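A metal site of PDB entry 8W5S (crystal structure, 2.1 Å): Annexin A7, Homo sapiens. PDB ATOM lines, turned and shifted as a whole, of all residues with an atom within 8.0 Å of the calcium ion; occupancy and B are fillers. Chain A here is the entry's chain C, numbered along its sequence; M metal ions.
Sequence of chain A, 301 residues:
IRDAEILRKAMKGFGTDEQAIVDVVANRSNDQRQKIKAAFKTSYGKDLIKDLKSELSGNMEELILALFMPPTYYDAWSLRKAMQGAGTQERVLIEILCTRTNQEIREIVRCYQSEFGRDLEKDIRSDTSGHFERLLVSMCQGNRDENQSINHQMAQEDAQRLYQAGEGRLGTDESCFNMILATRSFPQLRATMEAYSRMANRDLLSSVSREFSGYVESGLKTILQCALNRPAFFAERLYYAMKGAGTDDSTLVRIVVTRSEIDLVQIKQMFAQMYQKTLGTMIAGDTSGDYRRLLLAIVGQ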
ATOM      1  N   TYR A 163      19.980  24.075  27.690  1.00  0.00           N
ATOM      2  CA  TYR A 163      19.926  24.425  26.271  1.00  0.00           C
ATOM      3  C   TYR A 163      21.316  24.763  25.740  1.00  0.00           C
ATOM      4  O   TYR A 163      21.725  24.263  24.693  1.00  0.00           O
ATOM      5  CB  TYR A 163      18.969  25.597  26.053  1.00  0.00           C
ATOM      6  CG  TYR A 163      18.714  25.861  24.585  1.00  0.00           C
ATOM      7  CD1 TYR A 163      17.687  25.211  23.918  1.00  0.00           C
ATOM      8  CD2 TYR A 163      19.509  26.747  23.874  1.00  0.00           C
ATOM      9  CE1 TYR A 163      17.453  25.435  22.580  1.00  0.00           C
ATOM     10  CE2 TYR A 163      19.280  26.984  22.533  1.00  0.00           C
ATOM     11  CZ  TYR A 163      18.251  26.326  21.892  1.00  0.00           C
ATOM     12  OH  TYR A 163      18.022  26.563  20.551  1.00  0.00           O
ATOM     13  N   GLN A 164      22.046  25.611  26.458  1.00  0.00           N
ATOM     14  CA  GLN A 164      23.364  26.032  25.997  1.00  0.00           C
ATOM     15  C   GLN A 164      24.347  24.876  25.950  1.00  0.00           C
ATOM     16  O   GLN A 164      25.279  24.883  25.131  1.00  0.00           O
ATOM     17  CB  GLN A 164      23.892  27.165  26.889  1.00  0.00           C
ATOM     18  CG  GLN A 164      25.351  27.564  26.679  1.00  0.00           C
ATOM     19  CD  GLN A 164      25.700  27.862  25.224  1.00  0.00           C
ATOM     20  OE1 GLN A 164      24.852  28.268  24.435  1.00  0.00           O
ATOM     21  NE2 GLN A 164      26.966  27.655  24.879  1.00  0.00           N
ATOM     22  N   ALA A 165      24.158  23.857  26.791  1.00  0.00           N
ATOM     23  CA  ALA A 165      25.043  22.709  26.821  1.00  0.00           C
ATOM     24  C   ALA A 165      24.716  21.663  25.765  1.00  0.00           C
ATOM     25  O   ALA A 165      25.552  20.799  25.486  1.00  0.00           O
ATOM     26  CB  ALA A 165      25.029  22.056  28.207  1.00  0.00           C
ATOM     27  N   GLY A 166      23.529  21.719  25.173  1.00  0.00           N
ATOM     28  CA  GLY A 166      23.137  20.724  24.193  1.00  0.00           C
ATOM     29  C   GLY A 166      22.756  21.288  22.849  1.00  0.00           C
ATOM     30  O   GLY A 166      23.567  21.295  21.913  1.00  0.00           O
ATOM     31  N   GLU A 167      21.508  21.741  22.718  1.00  0.00           N
ATOM     32  CA  GLU A 167      20.997  22.204  21.435  1.00  0.00           C
ATOM     33  C   GLU A 167      21.773  23.419  20.942  1.00  0.00           C
ATOM     34  O   GLU A 167      22.308  23.422  19.829  1.00  0.00           O
ATOM     35  CB  GLU A 167      19.507  22.529  21.550  1.00  0.00           C
ATOM     36  CG  GLU A 167      18.658  21.367  22.039  1.00  0.00           C
ATOM     37  CD  GLU A 167      17.926  20.681  20.909  1.00  0.00           C
ATOM     38  OE1 GLU A 167      18.075  21.131  19.755  1.00  0.00           O
ATOM     39  OE2 GLU A 167      17.217  19.685  21.164  1.00  0.00           O
ATOM     40  N   GLY A 168      21.851  24.458  21.763  1.00  0.00           N
ATOM     41  CA  GLY A 168      22.426  25.723  21.345  1.00  0.00           C
ATOM     42  C   GLY A 168      23.931  25.730  21.194  1.00  0.00           C
ATOM     43  O   GLY A 168      24.537  26.800  21.108  1.00  0.00           O
ATOM     44  N   ARG A 169      24.562  24.561  21.154  1.00  0.00           N
ATOM     45  CA  ARG A 169      25.998  24.473  20.996  1.00  0.00           C
ATOM     46  C   ARG A 169      26.366  23.259  20.161  1.00  0.00           C
ATOM     47  O   ARG A 169      25.696  22.222  20.209  1.00  0.00           O
ATOM     48  CB  ARG A 169      26.722  24.431  22.350  1.00  0.00           C
ATOM     49  CG  ARG A 169      26.834  23.046  22.986  1.00  0.00           C
ATOM     50  CD  ARG A 169      27.788  23.071  24.166  1.00  0.00           C
ATOM     51  NE  ARG A 169      29.068  22.473  23.850  1.00  0.00           N
ATOM     52  CZ  ARG A 169      30.229  22.850  24.386  1.00  0.00           C
ATOM     53  NH1 ARG A 169      30.292  23.839  25.259  1.00  0.00           N
ATOM     54  NH2 ARG A 169      31.347  22.211  24.037  1.00  0.00           N
ATOM     55  N   LEU A 170      27.439  23.409  19.380  1.00  0.00           N
ATOM     56  CA  LEU A 170      27.959  22.297  18.594  1.00  0.00           C
ATOM     57  C   LEU A 170      28.431  21.186  19.527  1.00  0.00           C
ATOM     58  O   LEU A 170      29.063  21.444  20.553  1.00  0.00           O
ATOM     59  CB  LEU A 170      29.111  22.778  17.715  1.00  0.00           C
ATOM     60  CG  LEU A 170      29.829  21.753  16.838  1.00  0.00           C
ATOM     61  CD1 LEU A 170      29.082  21.525  15.536  1.00  0.00           C
ATOM     62  CD2 LEU A 170      31.258  22.215  16.569  1.00  0.00           C
ATOM     63  N   GLY A 171      28.107  19.951  19.168  1.00  0.00           N
ATOM     64  CA  GLY A 171      28.420  18.875  20.095  1.00  0.00           C
ATOM     65  C   GLY A 171      27.552  18.972  21.333  1.00  0.00           C
ATOM     66  O   GLY A 171      26.428  19.493  21.314  1.00  0.00           O
ATOM     67  N   THR A 172      28.088  18.477  22.447  1.00  0.00           N
ATOM     68  CA  THR A 172      27.337  18.487  23.705  1.00  0.00           C
ATOM     69  C   THR A 172      28.299  18.628  24.872  1.00  0.00           C
ATOM     70  O   THR A 172      29.357  17.985  24.898  1.00  0.00           O
ATOM     71  CB  THR A 172      26.510  17.209  23.864  1.00  0.00           C
ATOM     72  OG1 THR A 172      25.660  17.038  22.725  1.00  0.00           O
ATOM     73  CG2 THR A 172      25.652  17.284  25.119  1.00  0.00           C
ATOM     74  N   ASP A 173      27.937  19.488  25.826  1.00  0.00           N
ATOM     75  CA  ASP A 173      28.603  19.533  27.119  1.00  0.00           C
ATOM     76  C   ASP A 173      27.900  18.506  28.011  1.00  0.00           C
ATOM     77  O   ASP A 173      27.018  18.824  28.816  1.00  0.00           O
ATOM     78  CB  ASP A 173      28.542  20.939  27.715  1.00  0.00           C
ATOM     79  CG  ASP A 173      29.280  21.047  29.044  1.00  0.00           C
ATOM     80  OD1 ASP A 173      29.817  20.029  29.536  1.00  0.00           O
ATOM     81  OD2 ASP A 173      29.320  22.162  29.597  1.00  0.00           O
ATOM     82  N   PHE A 177      24.807  18.394  31.666  1.00  0.00           N
ATOM     83  CA  PHE A 177      23.630  17.554  31.870  1.00  0.00           C
ATOM     84  C   PHE A 177      23.786  16.716  33.129  1.00  0.00           C
ATOM     85  O   PHE A 177      22.859  16.614  33.945  1.00  0.00           O
ATOM     86  CB  PHE A 177      23.413  16.652  30.660  1.00  0.00           C
ATOM     87  CG  PHE A 177      22.615  17.290  29.555  1.00  0.00           C
ATOM     88  CD1 PHE A 177      23.211  18.180  28.680  1.00  0.00           C
ATOM     89  CD2 PHE A 177      21.274  16.989  29.402  1.00  0.00           C
ATOM     90  CE1 PHE A 177      22.481  18.760  27.666  1.00  0.00           C
ATOM     91  CE2 PHE A 177      20.536  17.564  28.386  1.00  0.00           C
ATOM     92  CZ  PHE A 177      21.140  18.459  27.513  1.00  0.00           C
ATOM     93  N   SER A 207      15.302  16.525  23.872  1.00  0.00           N
ATOM     94  CA  SER A 207      16.629  17.061  23.609  1.00  0.00           C
ATOM     95  C   SER A 207      17.709  16.028  23.893  1.00  0.00           C
ATOM     96  O   SER A 207      18.648  15.856  23.100  1.00  0.00           O
ATOM     97  CB  SER A 207      16.867  18.317  24.430  1.00  0.00           C
ATOM     98  OG  SER A 207      16.157  19.420  23.900  1.00  0.00           O
ATOM     99  N   ARG A 210      18.358  13.465  21.258  1.00  0.00           N
ATOM    100  CA  ARG A 210      19.087  14.021  20.119  1.00  0.00           C
ATOM    101  C   ARG A 210      20.499  14.455  20.472  1.00  0.00           C
ATOM    102  O   ARG A 210      21.376  14.414  19.608  1.00  0.00           O
ATOM    103  CB  ARG A 210      18.317  15.207  19.542  1.00  0.00           C
ATOM    104  CG  ARG A 210      16.825  14.964  19.389  1.00  0.00           C
ATOM    105  CD  ARG A 210      16.075  16.267  19.275  1.00  0.00           C
ATOM    106  NE  ARG A 210      16.361  16.917  18.005  1.00  0.00           N
ATOM    107  CZ  ARG A 210      16.562  18.219  17.855  1.00  0.00           C
ATOM    108  NH1 ARG A 210      16.503  19.046  18.883  1.00  0.00           N
ATOM    109  NH2 ARG A 210      16.849  18.702  16.650  1.00  0.00           N
ATOM    110  N   GLU A 211      20.734  14.873  21.709  1.00  0.00           N
ATOM    111  CA  GLU A 211      22.045  15.363  22.115  1.00  0.00           C
ATOM    112  C   GLU A 211      22.982  14.251  22.553  1.00  0.00           C
ATOM    113  O   GLU A 211      24.205  14.385  22.384  1.00  0.00           O
ATOM    114  CB  GLU A 211      21.894  16.374  23.253  1.00  0.00           C
ATOM    115  CG  GLU A 211      21.520  17.760  22.779  1.00  0.00           C
ATOM    116  CD  GLU A 211      22.541  18.332  21.821  1.00  0.00           C
ATOM    117  OE1 GLU A 211      23.753  18.190  22.084  1.00  0.00           O
ATOM    118  OE2 GLU A 211      22.139  18.941  20.803  1.00  0.00           O
ATOM    119  N   PHE A 212      22.457  13.171  23.110  1.00  0.00           N
ATOM    120  CA  PHE A 212      23.263  12.066  23.609  1.00  0.00           C
ATOM    121  C   PHE A 212      23.026  10.814  22.774  1.00  0.00           C
ATOM    122  O   PHE A 212      22.210  10.791  21.845  1.00  0.00           O
ATOM    123  CB  PHE A 212      22.963  11.800  25.075  1.00  0.00           C
ATOM    124  CG  PHE A 212      23.346  12.919  25.993  1.00  0.00           C
ATOM    125  CD1 PHE A 212      24.599  12.952  26.568  1.00  0.00           C
ATOM    126  CD2 PHE A 212      22.452  13.936  26.279  1.00  0.00           C
ATOM    127  CE1 PHE A 212      24.959  13.972  27.406  1.00  0.00           C
ATOM    128  CE2 PHE A 212      22.807  14.960  27.125  1.00  0.00           C
ATOM    129  CZ  PHE A 212      24.073  14.978  27.690  1.00  0.00           C
HETATM  130 CA    CA M   1      24.475  19.978  20.252  1.00  0.00          CA
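The calcium ion is bound by the backbone carbonyl oxygen (O) of Gly 171 (2.3 Å), the backbone carbonyl oxygen (O) of Gly 166 (2.3 Å), the backbone carbonyl oxygen (O) of Arg 169 (2.6 Å), the side-chain carboxylate (OE2) of Glu 211 (2.6 Å) and the side-chain carboxylate (OE1) of Glu 211 (2.7 Å).
Of the 16 residues printed, 4 come within 4 Å of the calcium ion. The nearest printed residue that does not touch the calcium ion is Thr 172 (4.02 Å).
The side-chain hydroxyl (OG1) of Thr 172 lies within hydrogen-bond range of the backbone carbonyl oxygen (O) of Glu 211 (3.0 Å). The backbone NH of Glu 167 sits close to the side-chain carboxylate of Glu 211.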
